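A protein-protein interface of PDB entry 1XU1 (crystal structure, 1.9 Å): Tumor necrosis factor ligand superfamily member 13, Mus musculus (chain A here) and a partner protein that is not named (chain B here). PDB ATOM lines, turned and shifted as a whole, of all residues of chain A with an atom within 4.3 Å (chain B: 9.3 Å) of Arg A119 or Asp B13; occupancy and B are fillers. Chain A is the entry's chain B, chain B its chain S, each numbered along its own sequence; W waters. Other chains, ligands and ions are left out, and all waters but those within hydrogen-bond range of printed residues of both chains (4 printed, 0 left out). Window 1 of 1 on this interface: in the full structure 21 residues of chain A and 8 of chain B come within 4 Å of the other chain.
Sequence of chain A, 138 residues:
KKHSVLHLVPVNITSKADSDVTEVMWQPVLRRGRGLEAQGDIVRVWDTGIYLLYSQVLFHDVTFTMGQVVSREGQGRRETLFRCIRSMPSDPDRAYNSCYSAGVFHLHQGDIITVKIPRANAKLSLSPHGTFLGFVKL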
ATOM      1  N   ASP A  20      16.077   4.086  -8.094  1.00  0.00           N
ATOM      2  CA  ASP A  20      16.305   2.907  -8.928  1.00  0.00           C
ATOM      3  C   ASP A  20      15.029   2.070  -8.963  1.00  0.00           C
ATOM      4  O   ASP A  20      15.047   0.847  -8.809  1.00  0.00           O
ATOM      5  CB  ASP A  20      17.497   2.117  -8.379  1.00  0.00           C
ATOM      6  CG  ASP A  20      18.800   2.884  -8.504  1.00  0.00           C
ATOM      7  OD1 ASP A  20      19.175   3.238  -9.651  1.00  0.00           O
ATOM      8  OD2 ASP A  20      19.513   3.189  -7.522  1.00  0.00           O
ATOM      9  N   VAL A  21      13.901   2.735  -9.186  1.00  0.00           N
ATOM     10  CA  VAL A  21      12.623   2.042  -9.204  1.00  0.00           C
ATOM     11  C   VAL A  21      11.661   2.665 -10.215  1.00  0.00           C
ATOM     12  O   VAL A  21      11.640   3.871 -10.415  1.00  0.00           O
ATOM     13  CB  VAL A  21      11.981   2.020  -7.772  1.00  0.00           C
ATOM     14  CG1 VAL A  21      11.688   3.414  -7.283  1.00  0.00           C
ATOM     15  CG2 VAL A  21      10.711   1.206  -7.746  1.00  0.00           C
ATOM     16  N   THR A  22      10.876   1.808 -10.841  1.00  0.00           N
ATOM     17  CA  THR A  22       9.812   2.201 -11.735  1.00  0.00           C
ATOM     18  C   THR A  22       8.518   1.593 -11.196  1.00  0.00           C
ATOM     19  O   THR A  22       8.481   0.413 -10.824  1.00  0.00           O
ATOM     20  CB  THR A  22      10.108   1.667 -13.145  1.00  0.00           C
ATOM     21  OG1 THR A  22      11.334   2.244 -13.625  1.00  0.00           O
ATOM     22  CG2 THR A  22       9.047   2.125 -14.145  1.00  0.00           C
ATOM     23  N   PHE A  64      20.022  -6.812 -18.088  1.00  0.00           N
ATOM     24  CA  PHE A  64      20.410  -8.218 -17.925  1.00  0.00           C
ATOM     25  C   PHE A  64      19.323  -9.094 -17.296  1.00  0.00           C
ATOM     26  O   PHE A  64      19.078 -10.221 -17.772  1.00  0.00           O
ATOM     27  CB  PHE A  64      21.765  -8.334 -17.200  1.00  0.00           C
ATOM     28  CG  PHE A  64      21.696  -8.158 -15.695  1.00  0.00           C
ATOM     29  CD1 PHE A  64      21.432  -6.917 -15.129  1.00  0.00           C
ATOM     30  CD2 PHE A  64      21.914  -9.243 -14.846  1.00  0.00           C
ATOM     31  CE1 PHE A  64      21.370  -6.764 -13.745  1.00  0.00           C
ATOM     32  CE2 PHE A  64      21.880  -9.086 -13.451  1.00  0.00           C
ATOM     33  CZ  PHE A  64      21.598  -7.849 -12.905  1.00  0.00           C
ATOM     34  N   THR A  65      18.650  -8.559 -16.277  1.00  0.00           N
ATOM     35  CA  THR A  65      17.450  -9.143 -15.727  1.00  0.00           C
ATOM     36  C   THR A  65      16.438  -8.045 -15.492  1.00  0.00           C
ATOM     37  O   THR A  65      16.790  -6.894 -15.203  1.00  0.00           O
ATOM     38  CB  THR A  65      17.701  -9.876 -14.368  1.00  0.00           C
ATOM     39  OG1 THR A  65      18.427  -9.019 -13.465  1.00  0.00           O
ATOM     40  CG2 THR A  65      18.569 -11.093 -14.555  1.00  0.00           C
ATOM     41  N   MET A  66      15.186  -8.417 -15.672  1.00  0.00           N
ATOM     42  CA  MET A  66      14.051  -7.550 -15.407  1.00  0.00           C
ATOM     43  C   MET A  66      13.018  -8.360 -14.651  1.00  0.00           C
ATOM     44  O   MET A  66      13.051  -9.575 -14.629  1.00  0.00           O
ATOM     45  CB  MET A  66      13.453  -7.018 -16.711  1.00  0.00           C
ATOM     46  CG  MET A  66      14.350  -6.031 -17.456  1.00  0.00           C
ATOM     47  SD  MET A  66      14.801  -4.524 -16.510  1.00  0.00           S
ATOM     48  CE  MET A  66      13.238  -3.687 -16.537  1.00  0.00           C
ATOM     49  N   ILE A 117       9.210  -2.278 -10.155  1.00  0.00           N
ATOM     50  CA  ILE A 117      10.291  -2.795 -10.982  1.00  0.00           C
ATOM     51  C   ILE A 117      11.561  -2.118 -10.455  1.00  0.00           C
ATOM     52  O   ILE A 117      11.700  -0.902 -10.586  1.00  0.00           O
ATOM     53  CB  ILE A 117      10.057  -2.480 -12.488  1.00  0.00           C
ATOM     54  CG1 ILE A 117       8.839  -3.229 -13.043  1.00  0.00           C
ATOM     55  CG2 ILE A 117      11.276  -2.894 -13.308  1.00  0.00           C
ATOM     56  CD1 ILE A 117       7.522  -2.669 -12.666  1.00  0.00           C
ATOM     57  N   PRO A 118      12.469  -2.862  -9.815  1.00  0.00           N
ATOM     58  CA  PRO A 118      13.671  -2.262  -9.228  1.00  0.00           C
ATOM     59  C   PRO A 118      14.785  -1.847 -10.211  1.00  0.00           C
ATOM     60  O   PRO A 118      15.960  -2.150  -9.999  1.00  0.00           O
ATOM     61  CB  PRO A 118      14.156  -3.359  -8.276  1.00  0.00           C
ATOM     62  CG  PRO A 118      13.020  -4.224  -8.111  1.00  0.00           C
ATOM     63  CD  PRO A 118      12.408  -4.296  -9.494  1.00  0.00           C
ATOM     64  N   ARG A 119      14.402  -1.164 -11.286  1.00  0.00           N
ATOM     65  CA  ARG A 119      15.329  -0.456 -12.155  1.00  0.00           C
ATOM     66  C   ARG A 119      14.707   0.890 -12.514  1.00  0.00           C
ATOM     67  O   ARG A 119      13.505   0.962 -12.758  1.00  0.00           O
ATOM     68  CB  ARG A 119      15.564  -1.238 -13.446  1.00  0.00           C
ATOM     69  CG  ARG A 119      16.396  -2.488 -13.269  1.00  0.00           C
ATOM     70  CD  ARG A 119      15.577  -3.712 -13.014  1.00  0.00           C
ATOM     71  NE  ARG A 119      16.382  -4.925 -13.042  1.00  0.00           N
ATOM     72  CZ  ARG A 119      17.138  -5.358 -12.040  1.00  0.00           C
ATOM     73  NH1 ARG A 119      17.213  -4.685 -10.892  1.00  0.00           N
ATOM     74  NH2 ARG A 119      17.822  -6.487 -12.180  1.00  0.00           N
ATOM     75  N   ALA A 120      15.535   1.931 -12.560  1.00  0.00           N
ATOM     76  CA  ALA A 120      15.113   3.254 -13.022  1.00  0.00           C
ATOM     77  C   ALA A 120      14.824   3.199 -14.518  1.00  0.00           C
ATOM     78  O   ALA A 120      15.523   2.521 -15.263  1.00  0.00           O
ATOM     79  CB  ALA A 120      16.186   4.277 -12.738  1.00  0.00           C
ATOM     80  N   ASN A 121      13.770   3.888 -14.949  1.00  0.00           N
ATOM     81  CA  ASN A 121      13.454   4.009 -16.365  1.00  0.00           C
ATOM     82  C   ASN A 121      13.330   2.642 -17.053  1.00  0.00           C
ATOM     83  O   ASN A 121      13.898   2.416 -18.131  1.00  0.00           O
ATOM     84  CB  ASN A 121      14.515   4.876 -17.056  1.00  0.00           C
ATOM     85  CG  ASN A 121      14.737   6.209 -16.342  1.00  0.00           C
ATOM     86  OD1 ASN A 121      15.874   6.627 -16.104  1.00  0.00           O
ATOM     87  ND2 ASN A 121      13.647   6.877 -16.001  1.00  0.00           N
ATOM     88  N   ALA A 122      12.593   1.733 -16.413  1.00  0.00           N
ATOM     89  CA  ALA A 122      12.334   0.415 -16.975  1.00  0.00           C
ATOM     90  C   ALA A 122      11.470   0.572 -18.227  1.00  0.00           C
ATOM     91  O   ALA A 122      10.560   1.405 -18.271  1.00  0.00           O
ATOM     92  CB  ALA A 122      11.637  -0.490 -15.955  1.00  0.00           C
ATOM     93  N   CYS B   4      28.527  -5.550   0.650  1.00  0.00           N
ATOM     94  CA  CYS B   4      28.388  -5.141  -0.781  1.00  0.00           C
ATOM     95  C   CYS B   4      29.045  -3.774  -1.000  1.00  0.00           C
ATOM     96  O   CYS B   4      28.426  -2.725  -0.790  1.00  0.00           O
ATOM     97  CB  CYS B   4      26.916  -5.117  -1.193  1.00  0.00           C
ATOM     98  SG  CYS B   4      26.635  -5.131  -2.981  1.00  0.00           S
ATOM     99  N   LYS B  10      30.483  -2.765  -7.286  1.00  0.00           N
ATOM    100  CA  LYS B  10      29.325  -3.623  -7.060  1.00  0.00           C
ATOM    101  C   LYS B  10      28.129  -2.806  -6.608  1.00  0.00           C
ATOM    102  O   LYS B  10      28.278  -1.754  -5.984  1.00  0.00           O
ATOM    103  CB  LYS B  10      29.636  -4.692  -6.012  1.00  0.00           C
ATOM    104  CG  LYS B  10      30.847  -5.561  -6.336  1.00  0.00           C
ATOM    105  CD  LYS B  10      31.387  -6.264  -5.094  1.00  0.00           C
ATOM    106  CE  LYS B  10      31.369  -7.774  -5.257  1.00  0.00           C
ATOM    107  NZ  LYS B  10      29.985  -8.300  -5.449  1.00  0.00           N
ATOM    108  N   PHE B  11      26.939  -3.298  -6.930  1.00  0.00           N
ATOM    109  CA  PHE B  11      25.707  -2.709  -6.423  1.00  0.00           C
ATOM    110  C   PHE B  11      24.804  -3.803  -5.874  1.00  0.00           C
ATOM    111  O   PHE B  11      24.909  -4.960  -6.271  1.00  0.00           O
ATOM    112  CB  PHE B  11      25.004  -1.911  -7.527  1.00  0.00           C
ATOM    113  CG  PHE B  11      24.316  -2.760  -8.563  1.00  0.00           C
ATOM    114  CD1 PHE B  11      25.042  -3.363  -9.583  1.00  0.00           C
ATOM    115  CD2 PHE B  11      22.935  -2.943  -8.525  1.00  0.00           C
ATOM    116  CE1 PHE B  11      24.404  -4.136 -10.547  1.00  0.00           C
ATOM    117  CE2 PHE B  11      22.293  -3.707  -9.483  1.00  0.00           C
ATOM    118  CZ  PHE B  11      23.027  -4.311 -10.492  1.00  0.00           C
ATOM    119  N   TYR B  12      23.954  -3.442  -4.923  1.00  0.00           N
ATOM    120  CA  TYR B  12      22.955  -4.365  -4.411  1.00  0.00           C
ATOM    121  C   TYR B  12      21.709  -4.307  -5.298  1.00  0.00           C
ATOM    122  O   TYR B  12      21.086  -3.268  -5.448  1.00  0.00           O
ATOM    123  CB  TYR B  12      22.599  -4.060  -2.964  1.00  0.00           C
ATOM    124  CG  TYR B  12      21.748  -5.149  -2.367  1.00  0.00           C
ATOM    125  CD1 TYR B  12      22.320  -6.335  -1.909  1.00  0.00           C
ATOM    126  CD2 TYR B  12      20.367  -5.019  -2.308  1.00  0.00           C
ATOM    127  CE1 TYR B  12      21.533  -7.352  -1.383  1.00  0.00           C
ATOM    128  CE2 TYR B  12      19.570  -6.024  -1.777  1.00  0.00           C
ATOM    129  CZ  TYR B  12      20.156  -7.187  -1.321  1.00  0.00           C
ATOM    130  OH  TYR B  12      19.364  -8.179  -0.806  1.00  0.00           O
ATOM    131  N   ASP B  13      21.367  -5.435  -5.892  1.00  0.00           N
ATOM    132  CA  ASP B  13      20.250  -5.521  -6.820  1.00  0.00           C
ATOM    133  C   ASP B  13      19.017  -5.887  -6.003  1.00  0.00           C
ATOM    134  O   ASP B  13      18.937  -6.994  -5.478  1.00  0.00           O
ATOM    135  CB  ASP B  13      20.549  -6.580  -7.875  1.00  0.00           C
ATOM    136  CG  ASP B  13      19.572  -6.556  -9.041  1.00  0.00           C
ATOM    137  OD1 ASP B  13      18.352  -6.413  -8.806  1.00  0.00           O
ATOM    138  OD2 ASP B  13      19.925  -6.714 -10.234  1.00  0.00           O
ATOM    139  N   HIS B  14      18.076  -4.950  -5.885  1.00  0.00           N
ATOM    140  CA  HIS B  14      16.866  -5.162  -5.097  1.00  0.00           C
ATOM    141  C   HIS B  14      15.868  -6.124  -5.744  1.00  0.00           C
ATOM    142  O   HIS B  14      14.954  -6.573  -5.074  1.00  0.00           O
ATOM    143  CB  HIS B  14      16.173  -3.826  -4.781  1.00  0.00           C
ATOM    144  CG  HIS B  14      16.894  -3.002  -3.760  1.00  0.00           C
ATOM    145  ND1 HIS B  14      17.707  -1.941  -4.097  1.00  0.00           N
ATOM    146  CD2 HIS B  14      16.931  -3.091  -2.410  1.00  0.00           C
ATOM    147  CE1 HIS B  14      18.208  -1.405  -2.997  1.00  0.00           C
ATOM    148  NE2 HIS B  14      17.758  -2.087  -1.959  1.00  0.00           N
ATOM    149  N   LEU B  15      16.018  -6.410  -7.031  1.00  0.00           N
ATOM    150  CA  LEU B  15      15.215  -7.448  -7.678  1.00  0.00           C
ATOM    151  C   LEU B  15      15.773  -8.820  -7.369  1.00  0.00           C
ATOM    152  O   LEU B  15      15.027  -9.723  -7.018  1.00  0.00           O
ATOM    153  CB  LEU B  15      15.138  -7.244  -9.202  1.00  0.00           C
ATOM    154  CG  LEU B  15      14.321  -8.299  -9.959  1.00  0.00           C
ATOM    155  CD1 LEU B  15      12.851  -8.322  -9.563  1.00  0.00           C
ATOM    156  CD2 LEU B  15      14.476  -8.105 -11.455  1.00  0.00           C
ATOM    157  N   LEU B  16      17.086  -8.974  -7.511  1.00  0.00           N
ATOM    158  CA  LEU B  16      17.748 -10.268  -7.324  1.00  0.00           C
ATOM    159  C   LEU B  16      18.051 -10.573  -5.853  1.00  0.00           C
ATOM    160  O   LEU B  16      18.236 -11.730  -5.492  1.00  0.00           O
ATOM    161  CB  LEU B  16      19.034 -10.319  -8.155  1.00  0.00           C
ATOM    162  CG  LEU B  16      18.897 -10.013  -9.644  1.00  0.00           C
ATOM    163  CD1 LEU B  16      20.239 -10.131 -10.333  1.00  0.00           C
ATOM    164  CD2 LEU B  16      17.881 -10.916 -10.324  1.00  0.00           C
ATOM    165  N   ARG B  17      18.056  -9.544  -5.006  1.00  0.00           N
ATOM    166  CA  ARG B  17      18.463  -9.653  -3.597  1.00  0.00           C
ATOM    167  C   ARG B  17      19.868 -10.270  -3.460  1.00  0.00           C
ATOM    168  O   ARG B  17      20.089 -11.201  -2.687  1.00  0.00           O
ATOM    169  CB  ARG B  17      17.434 -10.433  -2.768  1.00  0.00           C
ATOM    170  CG  ARG B  17      16.004  -9.873  -2.858  1.00  0.00           C
ATOM    171  CD  ARG B  17      15.860  -8.471  -2.278  1.00  0.00           C
ATOM    172  NE  ARG B  17      14.524  -7.923  -2.483  1.00  0.00           N
ATOM    173  CZ  ARG B  17      13.499  -8.070  -1.643  1.00  0.00           C
ATOM    174  NH1 ARG B  17      13.613  -8.769  -0.513  1.00  0.00           N
ATOM    175  NH2 ARG B  17      12.340  -7.505  -1.945  1.00  0.00           N
ATOM    176  N   ASP B  18      20.802  -9.706  -4.219  1.00  0.00           N
ATOM    177  CA  ASP B  18      22.170 -10.226  -4.346  1.00  0.00           C
ATOM    178  C   ASP B  18      23.108  -9.080  -4.720  1.00  0.00           C
ATOM    179  O   ASP B  18      22.681  -8.092  -5.315  1.00  0.00           O
ATOM    180  CB  ASP B  18      22.215 -11.278  -5.466  1.00  0.00           C
ATOM    181  CG  ASP B  18      22.965 -12.549  -5.083  1.00  0.00           C
ATOM    182  OD1 ASP B  18      23.847 -12.519  -4.192  1.00  0.00           O
ATOM    183  OD2 ASP B  18      22.734 -13.635  -5.661  1.00  0.00           O
ATOM    184  N   CYS B  19      24.386  -9.221  -4.397  1.00  0.00           N
ATOM    185  CA  CYS B  19      25.390  -8.249  -4.817  1.00  0.00           C
ATOM    186  C   CYS B  19      25.839  -8.606  -6.233  1.00  0.00           C
ATOM    187  O   CYS B  19      26.208  -9.741  -6.497  1.00  0.00           O
ATOM    188  CB  CYS B  19      26.577  -8.240  -3.848  1.00  0.00           C
ATOM    189  SG  CYS B  19      27.556  -6.717  -3.891  1.00  0.00           S
ATOM    190  N   ILE B  20      25.771  -7.636  -7.141  1.00  0.00           N
ATOM    191  CA  ILE B  20      26.143  -7.835  -8.539  1.00  0.00           C
ATOM    192  C   ILE B  20      27.366  -6.973  -8.891  1.00  0.00           C
ATOM    193  O   ILE B  20      27.472  -5.820  -8.479  1.00  0.00           O
ATOM    194  CB  ILE B  20      24.956  -7.470  -9.465  1.00  0.00           C
ATOM    195  CG1 ILE B  20      23.702  -8.294  -9.111  1.00  0.00           C
ATOM    196  CG2 ILE B  20      25.335  -7.659 -10.921  1.00  0.00           C
ATOM    197  CD1 ILE B  20      23.795  -9.785  -9.460  1.00  0.00           C
ATOM    198  N   SER B  21      28.286  -7.544  -9.652  1.00  0.00           N
ATOM    199  CA  SER B  21      29.452  -6.796 -10.128  1.00  0.00           C
ATOM    200  C   SER B  21      29.106  -6.096 -11.443  1.00  0.00           C
ATOM    201  O   SER B  21      28.683  -6.748 -12.391  1.00  0.00           O
ATOM    202  CB  SER B  21      30.635  -7.739 -10.320  1.00  0.00           C
ATOM    203  OG  SER B  21      31.766  -7.034 -10.796  1.00  0.00           O
ATOM    204  N   ILE B  25      28.143  -7.129 -16.274  1.00  0.00           N
ATOM    205  CA  ILE B  25      26.921  -6.824 -17.022  1.00  0.00           C
ATOM    206  C   ILE B  25      26.954  -5.574 -17.913  1.00  0.00           C
ATOM    207  O   ILE B  25      25.905  -5.169 -18.416  1.00  0.00           O
ATOM    208  CB  ILE B  25      25.728  -6.741 -16.057  1.00  0.00           C
ATOM    209  CG1 ILE B  25      25.928  -5.640 -15.016  1.00  0.00           C
ATOM    210  CG2 ILE B  25      25.505  -8.086 -15.372  1.00  0.00           C
ATOM    211  CD1 ILE B  25      24.668  -5.276 -14.281  1.00  0.00           C
ATOM    212  N   GLN B  28      24.382  -4.318 -20.670  1.00  0.00           N
ATOM    213  CA  GLN B  28      23.029  -4.668 -20.233  1.00  0.00           C
ATOM    214  C   GLN B  28      22.839  -4.205 -18.786  1.00  0.00           C
ATOM    215  O   GLN B  28      22.120  -4.819 -18.010  1.00  0.00           O
ATOM    216  CB  GLN B  28      22.834  -6.176 -20.307  1.00  0.00           C
ATOM    217  CG  GLN B  28      22.870  -6.768 -21.704  1.00  0.00           C
ATOM    218  CD  GLN B  28      22.405  -8.215 -21.707  1.00  0.00           C
ATOM    219  OE1 GLN B  28      23.218  -9.128 -21.661  1.00  0.00           O
ATOM    220  NE2 GLN B  28      21.100  -8.420 -21.753  1.00  0.00           N
ATOM    221  N   HIS B  29      23.505  -3.120 -18.435  1.00  0.00           N
ATOM    222  CA  HIS B  29      23.581  -2.662 -17.052  1.00  0.00           C
ATOM    223  C   HIS B  29      22.415  -1.715 -16.727  1.00  0.00           C
ATOM    224  O   HIS B  29      21.951  -0.970 -17.598  1.00  0.00           O
ATOM    225  CB  HIS B  29      24.939  -1.973 -16.798  1.00  0.00           C
ATOM    226  CG  HIS B  29      25.179  -0.774 -17.665  1.00  0.00           C
ATOM    227  ND1 HIS B  29      25.349  -0.865 -19.029  1.00  0.00           N
ATOM    228  CD2 HIS B  29      25.259   0.542 -17.365  1.00  0.00           C
ATOM    229  CE1 HIS B  29      25.511   0.344 -19.535  1.00  0.00           C
ATOM    230  NE2 HIS B  29      25.473   1.215 -18.544  1.00  0.00           N
ATOM    231  N   PRO B  30      21.952  -1.718 -15.478  1.00  0.00           N
ATOM    232  CA  PRO B  30      20.951  -0.735 -15.050  1.00  0.00           C
ATOM    233  C   PRO B  30      21.657   0.561 -14.643  1.00  0.00           C
ATOM    234  O   PRO B  30      22.885   0.619 -14.685  1.00  0.00           O
ATOM    235  CB  PRO B  30      20.299  -1.405 -13.847  1.00  0.00           C
ATOM    236  CG  PRO B  30      21.378  -2.272 -13.258  1.00  0.00           C
ATOM    237  CD  PRO B  30      22.342  -2.617 -14.373  1.00  0.00           C
ATOM    238  N   LYS B  31      20.896   1.564 -14.227  1.00  0.00           N
ATOM    239  CA  LYS B  31      21.429   2.905 -13.981  1.00  0.00           C
ATOM    240  C   LYS B  31      22.462   2.971 -12.845  1.00  0.00           C
ATOM    241  O   LYS B  31      23.322   3.847 -12.856  1.00  0.00           O
ATOM    242  CB  LYS B  31      20.273   3.868 -13.715  1.00  0.00           C
ATOM    243  CG  LYS B  31      20.656   5.336 -13.604  1.00  0.00           C
ATOM    244  CD  LYS B  31      19.421   6.233 -13.528  1.00  0.00           C
ATOM    245  CE  LYS B  31      19.285   6.956 -12.178  1.00  0.00           C
ATOM    246  NZ  LYS B  31      19.681   8.387 -12.269  1.00  0.00           N
ATOM    247  N   GLN B  32      22.391   2.055 -11.874  1.00  0.00           N
ATOM    248  CA  GLN B  32      23.379   2.013 -10.775  1.00  0.00           C
ATOM    249  C   GLN B  32      24.809   1.843 -11.299  1.00  0.00           C
ATOM    250  O   GLN B  32      25.771   2.285 -10.667  1.00  0.00           O
ATOM    251  CB  GLN B  32      23.089   0.858  -9.805  1.00  0.00           C
ATOM    252  CG  GLN B  32      21.821   1.003  -8.989  1.00  0.00           C
ATOM    253  CD  GLN B  32      20.704   0.115  -9.492  1.00  0.00           C
ATOM    254  OE1 GLN B  32      20.447   0.053 -10.695  1.00  0.00           O
ATOM    255  NE2 GLN B  32      20.038  -0.576  -8.580  1.00  0.00           N
ATOM    256  N   CYS B  33      24.937   1.170 -12.442  1.00  0.00           N
ATOM    257  CA  CYS B  33      26.229   0.898 -13.071  1.00  0.00           C
ATOM    258  C   CYS B  33      26.626   1.898 -14.163  1.00  0.00           C
ATOM    259  O   CYS B  33      27.621   1.684 -14.842  1.00  0.00           O
ATOM    260  CB  CYS B  33      26.185  -0.504 -13.687  1.00  0.00           C
ATOM    261  SG  CYS B  33      26.083  -1.830 -12.462  1.00  0.00           S
HETATM  262  O   HOH W   1      17.844  -2.467  -7.559  1.00  0.00           O
HETATM  263  O   HOH W   2      15.898  -0.661  -6.746  1.00  0.00           O
HETATM  264  O   HOH W   3      18.387   1.580 -11.518  1.00  0.00           O
HETATM  265  O   HOH W   4      18.012   1.286 -15.092  1.00  0.00           O
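The side-chain carboxylate (OD2) of Asp B13 is in salt-bridge range of the guanidinium group (NH2) of Arg A119 (2.9 Å). N of Phe A64 is in hydrogen-bond range of O of Gln B28.
N of Asp B13 sits at hydrogen-bond distance from O of Asp B18, at 3.0 Å. The side-chain hydroxyl (OG1) of Thr A65 is in hydrogen-bond range of the guanidinium group (NH2) of Arg A119, 2.9 Å away. The backbone carbonyl oxygen of Asp A20 lies within hydrogen-bond range of the backbone NH of Arg A119 (3.3 Å). The backbone NH (N) of Leu B15 sits at hydrogen-bond distance from the side-chain carboxylate (OD1) of Asp B13, 2.9 Å away. The side-chain sulfur of Cys B4 is disulfide-bonded to the side-chain sulfur of Cys B19. The backbone carbonyl oxygen (O) of Arg A119 is in hydrogen-bond range of the side-chain hydroxyl (OG1) of Thr A22 (2.7 Å).
Among the printed residues, pairs that only touch across the chains: Asp A20 with Gln B32, Phe A64 with Asp B13, Phe A64 with Leu B16, Phe A64 with Ile B25, Thr A65 with Leu B16, Met A66 with Leu B15, Pro A118 with Leu B15, Arg A119 with Leu B15 and Ala A120 with Lys B31.
Arg A119 touches two residues of chain B. Of chain A, only Phe A64 (3.3 Å) and Arg A119 (2.9 Å) come within 4 Å of Asp B13. Thr A65 touches one residue of chain B. Pro A118 touches one residue of chain B. Printed residues of chain B within 4 Å of Met A66: Leu B15 (3.5 Å). Of the printed residues of chain A, Leu B16 touches Phe A64 (3.7 Å) and Thr A65 (3.7 Å). Of the printed residues of chain A, Gln B32 touches Asp A20. Arg B17 touches none of the printed residues of chain A. The nearest residue of chain B that does not touch Arg A119 is Pro B30 (4.1 Å). The nearest residue of chain A that does not touch Asp B13 is Thr A65 (4.2 Å). The nearest printed residue of chain A that does not touch Lys B31 is Asp A20 (4.3 Å).
Hydrophobic or aromatic side chains of chain B within 4 Å of the printed part of chain A: Leu B15, Leu B16 and Ile B25. Of the 12 printed residues of chain A, 7 touch a printed residue of chain B. Printed residues of chain A that touch a printed residue of chain B: Asp A20, Phe A64, Thr A65, Met A66, Pro A118, Arg A119 and Ala A120.
Water W3 lies within hydrogen-bond range of the side-chain carboxylate of Asp A20, the side-chain amide oxygen of Gln B32 and the backbone NH of Ala A120. Water W2 bridges O of Asp A20 (2.7 Å) and ND1 of His B14 (3.5 Å). Water W4 lies within hydrogen-bond range of the backbone carbonyl oxygen of Ala A120 (2.8 Å) and the backbone NH of Lys B31 (3.0 Å). Water W1 lies within hydrogen-bond range of the backbone NH (N) of His B14 (3.0 Å), the side-chain amide nitrogen (NE2) of Gln B32 (3.1 Å) and the backbone carbonyl oxygen (O) of Pro A118 (3.1 Å).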
